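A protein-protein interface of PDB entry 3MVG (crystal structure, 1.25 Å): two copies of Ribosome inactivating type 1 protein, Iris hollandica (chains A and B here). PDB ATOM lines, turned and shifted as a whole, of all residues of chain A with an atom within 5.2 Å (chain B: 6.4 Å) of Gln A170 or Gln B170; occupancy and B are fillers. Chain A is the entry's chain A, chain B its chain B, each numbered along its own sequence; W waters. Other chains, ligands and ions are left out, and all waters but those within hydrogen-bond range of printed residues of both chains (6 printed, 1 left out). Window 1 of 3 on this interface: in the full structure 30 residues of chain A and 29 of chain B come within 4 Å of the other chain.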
ATOM      1  N   ARG A 166      31.475  24.194 -36.296  1.00  0.00           N
ATOM      2  CA  ARG A 166      30.978  23.214 -35.339  1.00  0.00           C
ATOM      3  C   ARG A 166      30.568  23.859 -34.019  1.00  0.00           C
ATOM      4  O   ARG A 166      29.744  23.291 -33.293  1.00  0.00           O
ATOM      5  CB  ARG A 166      31.998  22.095 -35.125  1.00  0.00           C
ATOM      6  CG  ARG A 166      32.204  21.273 -36.376  1.00  0.00           C
ATOM      7  CD  ARG A 166      33.389  20.345 -36.267  1.00  0.00           C
ATOM      8  NE  ARG A 166      33.674  19.689 -37.538  1.00  0.00           N
ATOM      9  CZ  ARG A 166      33.077  18.583 -37.980  1.00  0.00           C
ATOM     10  NH1 ARG A 166      32.165  17.954 -37.238  1.00  0.00           N
ATOM     11  NH2 ARG A 166      33.400  18.118 -39.176  1.00  0.00           N
ATOM     12  N   ALA A 167      31.109  25.035 -33.705  1.00  0.00           N
ATOM     13  CA  ALA A 167      30.680  25.741 -32.494  1.00  0.00           C
ATOM     14  C   ALA A 167      29.217  26.154 -32.590  1.00  0.00           C
ATOM     15  O   ALA A 167      28.507  26.174 -31.580  1.00  0.00           O
ATOM     16  CB  ALA A 167      31.550  26.950 -32.226  1.00  0.00           C
ATOM     17  N   ILE A 168      28.764  26.481 -33.796  1.00  0.00           N
ATOM     18  CA  ILE A 168      27.352  26.824 -33.999  1.00  0.00           C
ATOM     19  C   ILE A 168      26.491  25.553 -34.006  1.00  0.00           C
ATOM     20  O   ILE A 168      25.427  25.521 -33.379  1.00  0.00           O
ATOM     21  CB  ILE A 168      27.131  27.700 -35.255  1.00  0.00           C
ATOM     22  CG1 ILE A 168      28.059  28.923 -35.206  1.00  0.00           C
ATOM     23  CG2 ILE A 168      25.651  28.118 -35.360  1.00  0.00           C
ATOM     24  CD1 ILE A 168      27.996  29.816 -36.434  1.00  0.00           C
ATOM     25  N   GLU A 169      26.950  24.508 -34.693  1.00  0.00           N
ATOM     26  CA  GLU A 169      26.310  23.195 -34.612  1.00  0.00           C
ATOM     27  C   GLU A 169      26.058  22.787 -33.158  1.00  0.00           C
ATOM     28  O   GLU A 169      24.970  22.318 -32.815  1.00  0.00           O
ATOM     29  CB  GLU A 169      27.180  22.148 -35.299  1.00  0.00           C
ATOM     30  CG  GLU A 169      26.628  20.749 -35.169  1.00  0.00           C
ATOM     31  CD  GLU A 169      27.511  19.702 -35.799  1.00  0.00           C
ATOM     32  OE1 GLU A 169      27.104  18.525 -35.829  1.00  0.00           O
ATOM     33  OE2 GLU A 169      28.610  20.044 -36.285  1.00  0.00           O
ATOM     34  N   GLN A 170      27.065  22.967 -32.308  1.00  0.00           N
ATOM     35  CA  GLN A 170      26.983  22.608 -30.889  1.00  0.00           C
ATOM     36  C   GLN A 170      25.800  23.266 -30.175  1.00  0.00           C
ATOM     37  O   GLN A 170      25.108  22.616 -29.369  1.00  0.00           O
ATOM     38  CB  GLN A 170      28.289  22.995 -30.191  1.00  0.00           C
ATOM     39  CG  GLN A 170      28.253  22.869 -28.697  1.00  0.00           C
ATOM     40  CD  GLN A 170      28.663  21.509 -28.239  1.00  0.00           C
ATOM     41  OE1 GLN A 170      28.032  20.501 -28.560  1.00  0.00           O
ATOM     42  NE2 GLN A 170      29.739  21.463 -27.495  1.00  0.00           N
ATOM     43  N   ARG A 171      25.583  24.549 -30.462  1.00  0.00           N
ATOM     44  CA  ARG A 171      24.463  25.294 -29.891  1.00  0.00           C
ATOM     45  C   ARG A 171      23.152  24.593 -30.232  1.00  0.00           C
ATOM     46  O   ARG A 171      22.277  24.439 -29.374  1.00  0.00           O
ATOM     47  CB  ARG A 171      24.430  26.734 -30.418  1.00  0.00           C
ATOM     48  CG  ARG A 171      25.727  27.518 -30.271  1.00  0.00           C
ATOM     49  CD  ARG A 171      26.292  27.392 -28.873  1.00  0.00           C
ATOM     50  NE  ARG A 171      27.163  28.512 -28.518  1.00  0.00           N
ATOM     51  CZ  ARG A 171      28.485  28.508 -28.645  1.00  0.00           C
ATOM     52  NH1 ARG A 171      29.106  27.445 -29.138  1.00  0.00           N
ATOM     53  NH2 ARG A 171      29.188  29.573 -28.281  1.00  0.00           N
ATOM     54  N   VAL A 172      23.028  24.167 -31.488  1.00  0.00           N
ATOM     55  CA  VAL A 172      21.832  23.484 -31.970  1.00  0.00           C
ATOM     56  C   VAL A 172      21.670  22.130 -31.283  1.00  0.00           C
ATOM     57  O   VAL A 172      20.608  21.825 -30.734  1.00  0.00           O
ATOM     58  CB  VAL A 172      21.853  23.320 -33.516  1.00  0.00           C
ATOM     59  CG1 VAL A 172      20.580  22.647 -34.003  1.00  0.00           C
ATOM     60  CG2 VAL A 172      22.005  24.673 -34.186  1.00  0.00           C
ATOM     61  N   THR A 173      22.712  21.308 -31.279  1.00  0.00           N
ATOM     62  CA  THR A 173      22.557  19.976 -30.692  1.00  0.00           C
ATOM     63  C   THR A 173      22.356  20.029 -29.178  1.00  0.00           C
ATOM     64  O   THR A 173      21.658  19.173 -28.636  1.00  0.00           O
ATOM     65  CB  THR A 173      23.688  19.019 -31.087  1.00  0.00           C
ATOM     66  OG1 THR A 173      24.926  19.560 -30.649  1.00  0.00           O
ATOM     67  CG2 THR A 173      23.732  18.833 -32.603  1.00  0.00           C
ATOM     68  N   ASN A 174      22.889  21.047 -28.509  1.00  0.00           N
ATOM     69  CA  ASN A 174      22.629  21.229 -27.072  1.00  0.00           C
ATOM     70  C   ASN A 174      21.158  21.503 -26.755  1.00  0.00           C
ATOM     71  O   ASN A 174      20.732  21.446 -25.599  1.00  0.00           O
ATOM     72  CB  ASN A 174      23.444  22.393 -26.530  1.00  0.00           C
ATOM     73  CG  ASN A 174      24.934  22.088 -26.416  1.00  0.00           C
ATOM     74  OD1 ASN A 174      25.374  20.956 -26.593  1.00  0.00           O
ATOM     75  ND2 ASN A 174      25.715  23.124 -26.145  1.00  0.00           N
ATOM     76  N   ASN A 175      20.393  21.835 -27.786  1.00  0.00           N
ATOM     77  CA  ASN A 175      18.986  22.148 -27.621  1.00  0.00           C
ATOM     78  C   ASN A 175      18.048  21.132 -28.248  1.00  0.00           C
ATOM     79  O   ASN A 175      16.840  21.353 -28.290  1.00  0.00           O
ATOM     80  CB  ASN A 175      18.735  23.572 -28.096  1.00  0.00           C
ATOM     81  CG  ASN A 175      19.203  24.571 -27.085  1.00  0.00           C
ATOM     82  OD1 ASN A 175      18.683  24.606 -25.966  1.00  0.00           O
ATOM     83  ND2 ASN A 175      20.220  25.359 -27.428  1.00  0.00           N
ATOM     84  N   THR A 240      39.702  24.039 -32.928  1.00  0.00           N
ATOM     85  CA  THR A 240      39.222  23.506 -31.646  1.00  0.00           C
ATOM     86  C   THR A 240      38.190  24.403 -30.966  1.00  0.00           C
ATOM     87  O   THR A 240      37.130  23.930 -30.548  1.00  0.00           O
ATOM     88  CB  THR A 240      40.396  23.267 -30.676  1.00  0.00           C
ATOM     89  OG1 THR A 240      41.312  22.348 -31.274  1.00  0.00           O
ATOM     90  CG2 THR A 240      39.930  22.694 -29.354  1.00  0.00           C
ATOM     91  N   THR B 162      33.860  15.718 -20.089  1.00  0.00           N
ATOM     92  CA  THR B 162      33.088  15.753 -21.318  1.00  0.00           C
ATOM     93  C   THR B 162      31.662  15.226 -21.095  1.00  0.00           C
ATOM     94  O   THR B 162      30.735  15.697 -21.744  1.00  0.00           O
ATOM     95  CB  THR B 162      33.776  14.950 -22.412  1.00  0.00           C
ATOM     96  OG1 THR B 162      34.066  13.654 -21.893  1.00  0.00           O
ATOM     97  CG2 THR B 162      35.075  15.630 -22.877  1.00  0.00           C
ATOM     98  N   PHE B 165      30.012  18.353 -19.590  1.00  0.00           N
ATOM     99  CA  PHE B 165      29.949  19.547 -20.446  1.00  0.00           C
ATOM    100  C   PHE B 165      30.120  19.218 -21.911  1.00  0.00           C
ATOM    101  O   PHE B 165      31.215  18.837 -22.353  1.00  0.00           O
ATOM    102  CB  PHE B 165      31.059  20.537 -20.083  1.00  0.00           C
ATOM    103  CG  PHE B 165      30.898  21.187 -18.748  1.00  0.00           C
ATOM    104  CD1 PHE B 165      29.994  22.224 -18.562  1.00  0.00           C
ATOM    105  CD2 PHE B 165      31.687  20.786 -17.679  1.00  0.00           C
ATOM    106  CE1 PHE B 165      29.868  22.838 -17.323  1.00  0.00           C
ATOM    107  CE2 PHE B 165      31.568  21.400 -16.436  1.00  0.00           C
ATOM    108  CZ  PHE B 165      30.663  22.430 -16.263  1.00  0.00           C
ATOM    109  N   ARG B 166      29.052  19.402 -22.683  1.00  0.00           N
ATOM    110  CA  ARG B 166      29.129  19.218 -24.128  1.00  0.00           C
ATOM    111  C   ARG B 166      30.088  20.213 -24.789  1.00  0.00           C
ATOM    112  O   ARG B 166      30.600  19.944 -25.878  1.00  0.00           O
ATOM    113  CB  ARG B 166      27.740  19.253 -24.773  1.00  0.00           C
ATOM    114  CG  ARG B 166      26.876  18.049 -24.412  1.00  0.00           C
ATOM    115  CD  ARG B 166      25.378  18.325 -24.643  1.00  0.00           C
ATOM    116  NE  ARG B 166      24.561  17.250 -24.083  1.00  0.00           N
ATOM    117  CZ  ARG B 166      24.336  16.085 -24.684  1.00  0.00           C
ATOM    118  NH1 ARG B 166      23.614  15.151 -24.073  1.00  0.00           N
ATOM    119  NH2 ARG B 166      24.853  15.844 -25.884  1.00  0.00           N
ATOM    120  N   ALA B 167      30.350  21.346 -24.135  1.00  0.00           N
ATOM    121  CA  ALA B 167      31.345  22.303 -24.653  1.00  0.00           C
ATOM    122  C   ALA B 167      32.746  21.687 -24.672  1.00  0.00           C
ATOM    123  O   ALA B 167      33.539  21.977 -25.564  1.00  0.00           O
ATOM    124  CB  ALA B 167      31.341  23.610 -23.872  1.00  0.00           C
ATOM    125  N   ILE B 168      33.050  20.840 -23.687  1.00  0.00           N
ATOM    126  CA  ILE B 168      34.341  20.159 -23.647  1.00  0.00           C
ATOM    127  C   ILE B 168      34.342  18.992 -24.643  1.00  0.00           C
ATOM    128  O   ILE B 168      35.316  18.796 -25.374  1.00  0.00           O
ATOM    129  CB  ILE B 168      34.727  19.722 -22.213  1.00  0.00           C
ATOM    130  CG1 ILE B 168      34.651  20.929 -21.265  1.00  0.00           C
ATOM    131  CG2 ILE B 168      36.132  19.100 -22.214  1.00  0.00           C
ATOM    132  CD1 ILE B 168      34.955  20.608 -19.817  1.00  0.00           C
ATOM    133  N   GLU B 169      33.240  18.240 -24.686  1.00  0.00           N
ATOM    134  CA  GLU B 169      33.059  17.220 -25.715  1.00  0.00           C
ATOM    135  C   GLU B 169      33.350  17.761 -27.116  1.00  0.00           C
ATOM    136  O   GLU B 169      34.028  17.104 -27.906  1.00  0.00           O
ATOM    137  CB  GLU B 169      31.638  16.658 -25.655  1.00  0.00           C
ATOM    138  CG  GLU B 169      31.282  15.746 -26.823  1.00  0.00           C
ATOM    139  CD  GLU B 169      29.852  15.254 -26.766  1.00  0.00           C
ATOM    140  OE1 GLU B 169      29.487  14.427 -27.632  1.00  0.00           O
ATOM    141  OE2 GLU B 169      29.084  15.676 -25.874  1.00  0.00           O
ATOM    142  N   GLN B 170      32.838  18.952 -27.412  1.00  0.00           N
ATOM    143  CA  GLN B 170      33.005  19.542 -28.737  1.00  0.00           C
ATOM    144  C   GLN B 170      34.470  19.751 -29.088  1.00  0.00           C
ATOM    145  O   GLN B 170      34.861  19.576 -30.242  1.00  0.00           O
ATOM    146  CB  GLN B 170      32.230  20.858 -28.845  1.00  0.00           C
ATOM    147  CG  GLN B 170      32.073  21.390 -30.285  1.00  0.00           C
ATOM    148  CD  GLN B 170      31.264  20.456 -31.197  1.00  0.00           C
ATOM    149  OE1 GLN B 170      31.747  20.009 -32.247  1.00  0.00           O
ATOM    150  NE2 GLN B 170      30.028  20.160 -30.800  1.00  0.00           N
ATOM    151  N   ARG B 171      35.287  20.134 -28.110  1.00  0.00           N
ATOM    152  CA  ARG B 171      36.716  20.313 -28.369  1.00  0.00           C
ATOM    153  C   ARG B 171      37.361  19.003 -28.804  1.00  0.00           C
ATOM    154  O   ARG B 171      38.249  18.992 -29.670  1.00  0.00           O
ATOM    155  CB  ARG B 171      37.430  20.878 -27.141  1.00  0.00           C
ATOM    156  CG  ARG B 171      36.793  22.120 -26.533  1.00  0.00           C
ATOM    157  CD  ARG B 171      36.864  23.311 -27.449  1.00  0.00           C
ATOM    158  NE  ARG B 171      36.254  24.497 -26.850  1.00  0.00           N
ATOM    159  CZ  ARG B 171      36.810  25.234 -25.891  1.00  0.00           C
ATOM    160  NH1 ARG B 171      38.000  24.918 -25.405  1.00  0.00           N
ATOM    161  NH2 ARG B 171      36.173  26.296 -25.414  1.00  0.00           N
ATOM    162  N   VAL B 172      36.906  17.905 -28.211  1.00  0.00           N
ATOM    163  CA  VAL B 172      37.379  16.574 -28.580  1.00  0.00           C
ATOM    164  C   VAL B 172      36.907  16.198 -29.990  1.00  0.00           C
ATOM    165  O   VAL B 172      37.703  15.781 -30.826  1.00  0.00           O
ATOM    166  CB  VAL B 172      36.927  15.508 -27.557  1.00  0.00           C
ATOM    167  CG1 VAL B 172      37.455  14.137 -27.939  1.00  0.00           C
ATOM    168  CG2 VAL B 172      37.371  15.886 -26.151  1.00  0.00           C
ATOM    169  N   THR B 173      35.609  16.369 -30.230  1.00  0.00           N
ATOM    170  CA  THR B 173      34.987  16.057 -31.512  1.00  0.00           C
ATOM    171  C   THR B 173      35.624  16.835 -32.665  1.00  0.00           C
ATOM    172  O   THR B 173      35.820  16.293 -33.755  1.00  0.00           O
ATOM    173  CB  THR B 173      33.472  16.313 -31.435  1.00  0.00           C
ATOM    174  OG1 THR B 173      32.857  15.270 -30.666  1.00  0.00           O
ATOM    175  CG2 THR B 173      32.861  16.351 -32.807  1.00  0.00           C
ATOM    176  N   ASN B 174      35.985  18.088 -32.397  1.00  0.00           N
ATOM    177  CA  ASN B 174      36.658  18.964 -33.367  1.00  0.00           C
ATOM    178  C   ASN B 174      38.052  18.480 -33.758  1.00  0.00           C
ATOM    179  O   ASN B 174      38.646  18.975 -34.728  1.00  0.00           O
ATOM    180  CB  ASN B 174      36.765  20.395 -32.835  1.00  0.00           C
ATOM    181  CG  ASN B 174      35.434  21.096 -32.764  1.00  0.00           C
ATOM    182  OD1 ASN B 174      34.435  20.616 -33.290  1.00  0.00           O
ATOM    183  ND2 ASN B 174      35.412  22.239 -32.096  1.00  0.00           N
ATOM    184  N   ASN B 175      38.570  17.520 -33.001  1.00  0.00           N
ATOM    185  CA  ASN B 175      39.894  16.993 -33.253  1.00  0.00           C
ATOM    186  C   ASN B 175      39.940  15.518 -33.624  1.00  0.00           C
ATOM    187  O   ASN B 175      41.022  14.940 -33.723  1.00  0.00           O
ATOM    188  CB  ASN B 175      40.798  17.335 -32.068  1.00  0.00           C
ATOM    189  CG  ASN B 175      41.213  18.775 -32.095  1.00  0.00           C
ATOM    190  OD1 ASN B 175      41.947  19.197 -32.990  1.00  0.00           O
ATOM    191  ND2 ASN B 175      40.711  19.556 -31.157  1.00  0.00           N
ATOM    192  N   ARG B 239      22.764  25.715 -20.747  1.00  0.00           N
ATOM    193  CA  ARG B 239      22.563  24.576 -21.614  1.00  0.00           C
ATOM    194  C   ARG B 239      23.201  24.799 -22.985  1.00  0.00           C
ATOM    195  O   ARG B 239      23.804  23.878 -23.549  1.00  0.00           O
ATOM    196  CB  ARG B 239      21.070  24.269 -21.730  1.00  0.00           C
ATOM    197  CG  ARG B 239      20.764  22.875 -22.263  1.00  0.00           C
ATOM    198  CD  ARG B 239      19.262  22.623 -22.384  1.00  0.00           C
ATOM    199  NE  ARG B 239      18.626  23.709 -23.124  1.00  0.00           N
ATOM    200  CZ  ARG B 239      17.710  24.541 -22.642  1.00  0.00           C
ATOM    201  NH1 ARG B 239      17.228  24.423 -21.405  1.00  0.00           N
ATOM    202  NH2 ARG B 239      17.251  25.498 -23.432  1.00  0.00           N
ATOM    203  N   THR B 240      23.081  26.017 -23.507  1.00  0.00           N
ATOM    204  CA  THR B 240      23.482  26.336 -24.882  1.00  0.00           C
ATOM    205  C   THR B 240      24.969  26.674 -25.016  1.00  0.00           C
ATOM    206  O   THR B 240      25.657  26.103 -25.871  1.00  0.00           O
ATOM    207  CB  THR B 240      22.606  27.478 -25.455  1.00  0.00           C
ATOM    208  OG1 THR B 240      21.226  27.098 -25.381  1.00  0.00           O
ATOM    209  CG2 THR B 240      22.954  27.781 -26.907  1.00  0.00           C
ATOM    210  N   PHE B 241      25.444  27.596 -24.180  1.00  0.00           N
ATOM    211  CA  PHE B 241      26.829  28.076 -24.215  1.00  0.00           C
ATOM    212  C   PHE B 241      27.797  27.103 -23.518  1.00  0.00           C
ATOM    213  O   PHE B 241      28.826  26.722 -24.083  1.00  0.00           O
ATOM    214  CB  PHE B 241      26.910  29.480 -23.596  1.00  0.00           C
ATOM    215  CG  PHE B 241      28.295  30.063 -23.574  1.00  0.00           C
ATOM    216  CD1 PHE B 241      28.838  30.644 -24.716  1.00  0.00           C
ATOM    217  CD2 PHE B 241      29.050  30.048 -22.408  1.00  0.00           C
ATOM    218  CE1 PHE B 241      30.123  31.186 -24.702  1.00  0.00           C
ATOM    219  CE2 PHE B 241      30.337  30.591 -22.382  1.00  0.00           C
ATOM    220  CZ  PHE B 241      30.870  31.165 -23.533  1.00  0.00           C
ATOM    221  N   CYS B 242      27.470  26.697 -22.296  1.00  0.00           N
ATOM    222  CA  CYS B 242      28.331  25.786 -21.537  1.00  0.00           C
ATOM    223  C   CYS B 242      28.155  24.337 -21.957  1.00  0.00           C
ATOM    224  O   CYS B 242      29.016  23.491 -21.688  1.00  0.00           O
ATOM    225  CB  CYS B 242      28.036  25.884 -20.041  1.00  0.00           C
ATOM    226  SG  CYS B 242      28.201  27.535 -19.356  1.00  0.00           S
ATOM    227  N   GLY B 243      27.034  24.026 -22.594  1.00  0.00           N
ATOM    228  CA  GLY B 243      26.689  22.634 -22.869  1.00  0.00           C
ATOM    229  C   GLY B 243      26.554  21.817 -21.594  1.00  0.00           C
ATOM    230  O   GLY B 243      26.869  20.632 -21.579  1.00  0.00           O
HETATM  231  O   HOH W   1      30.607  18.633 -34.866  1.00  0.00           O
HETATM  232  O   HOH W   2      27.481  19.318 -32.073  1.00  0.00           O
HETATM  233  O   HOH W   3      29.271  18.448 -28.070  1.00  0.00           O
HETATM  234  O   HOH W   4      17.890  27.066 -25.246  1.00  0.00           O
HETATM  235  O   HOH W   5      37.108  19.542 -36.907  1.00  0.00           O
HETATM  236  O   HOH W   6      33.655  24.462 -31.378  1.00  0.00           O
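The side-chain amide nitrogen (ND2) of Asn A174 is in hydrogen-bond range of the backbone carbonyl oxygen (O) of Thr B240 (3.0 Å).
The side-chain amide nitrogen (NE2) of Gln A170 sits close to the backbone carbonyl oxygen (O) of Arg B166 (2.4 Å).
The side-chain hydroxyl (OG1) of Thr B240 is in hydrogen-bond range of the side-chain amide nitrogen (ND2) of Asn A175 (2.9 Å).
NE of Arg B239 lies within hydrogen-bond range of OD1 of Asn A175 (3.0 Å).
ND2 of Asn A174 sits at hydrogen-bond distance from O of Arg B239, 3.3 Å away.
ND2 of Asn B175 sits at hydrogen-bond distance from OG1 of Thr A240 (2.9 Å).
NE2 of Gln A170 sits close to N of Ala B167 (3.4 Å).
O of Thr A240 lies within hydrogen-bond range of ND2 of Asn B174.
NE2 of Gln B170 lies within hydrogen-bond range of OE1 of Gln A170 (3.0 Å).
The backbone carbonyl oxygen (O) of Gln A170 sits at hydrogen-bond distance from the side-chain hydroxyl (OG1) of Thr A173, 3.3 Å away.
O of Gly B243 lies within hydrogen-bond range of N of Arg B166 (2.7 Å).
The backbone carbonyl oxygen (O) of Ala A167 is in hydrogen-bond range of the guanidinium group (NH1) of Arg A171, at 2.8 Å.
OE1 of Gln B170 sits close to OD1 of Asn B174, at 2.9 Å.
The backbone carbonyl oxygen of Gln A170 lies close to the side-chain amide oxygen of Asn A174, 3.2 Å away.
The side-chain amide nitrogen of Asn B175 is in hydrogen-bond range of the backbone carbonyl oxygen of Arg B171.
Arg A166 touches Gln B170.
Asn B174 touches Arg A166.
Thr B240 touches Arg A171 (O to CD, 3.3 Å).
Phe B241 touches Arg A171 (CD1 to NH2, 3.7 Å).
OD1 of Asn A174 touches CD of Arg B166, at 3.3 Å.
CA of Gly B243 touches ND2 of Asn A174, 3.5 Å away.
Arg B171 touches Thr A240 (CD to O, 3.2 Å).
Printed residues of chain B within 4 Å of Gln A170: Arg B166, Ala B167 and Gln B170.
Gln B170 touches two residues of chain A.
Printed residues of chain B within 4 Å of Arg A166: Gln B170 (3.6 Å) and Asn B174 (3.2 Å).
Printed residues of chain A within 4 Å of Arg B166: Gln A170 and Asn A174.
The nearest residue of chain A that does not touch Gln B170 is Thr A240 (4.9 Å).
Of the 17 printed residues of chain B, 10 touch a printed residue of chain A.
Printed residues of chain B that touch a printed residue of chain A: Arg B166, Ala B167, Gln B170, Arg B171, Asn B174, Asn B175, Arg B239, Thr B240, Phe B241 and Gly B243.
Hydrophobic or aromatic side chains of chain B within 4 Å of the printed part of chain A: Phe B241.
Along chain B the printed residues that touch a printed residue of chain A span positions 166 to 243.
Of the 11 printed residues of chain A, 6 touch a printed residue of chain B.
Among the printed residues, 16 pairs touch across the chains.
Arg A166 touches Gln B170, and with the chains exchanged Gln A170 touches Arg B166.
Arg A166 touches Asn B174, and with the chains exchanged Asn A174 touches Arg B166.
Asn A174 touches Thr B240, and with the chains exchanged Thr A240 touches Asn B174.
Asn A175 touches Thr B240, and with the chains exchanged Thr A240 touches Asn B175.
Positions printed for both chains: 166, 167, 168, 169, 170, 171, 172, 173, 174, 175 and 240.
Of the 16 pairs that touch across the chains among the printed residues, 11 have their exchanged pair printed and touching as well.
Water W3 lies within hydrogen-bond range of OE1 of Gln A170, O of Arg B166 and NE2 of Gln B170.
Water W4 lies within hydrogen-bond range of the guanidinium group (NH2) of Arg B239, the side-chain amide oxygen (OD1) of Asn A175 and the side-chain hydroxyl (OG1) of Thr B240.
Water W5 lies within hydrogen-bond range of the backbone carbonyl oxygen of Asn B174 and the guanidinium group of Arg A166.
Water W1 lies within hydrogen-bond range of the side-chain carboxylate of Glu A169, the guanidinium group of Arg A166 and the side-chain amide oxygen of Gln B170.
Water W6 lies within hydrogen-bond range of the side-chain amide nitrogen of Asn B174 (2.9 Å) and the backbone NH of Ala A167 (3.5 Å).
Water W2 bridges the side-chain hydroxyl of Thr A173 and the side-chain amide nitrogen of Gln B170.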
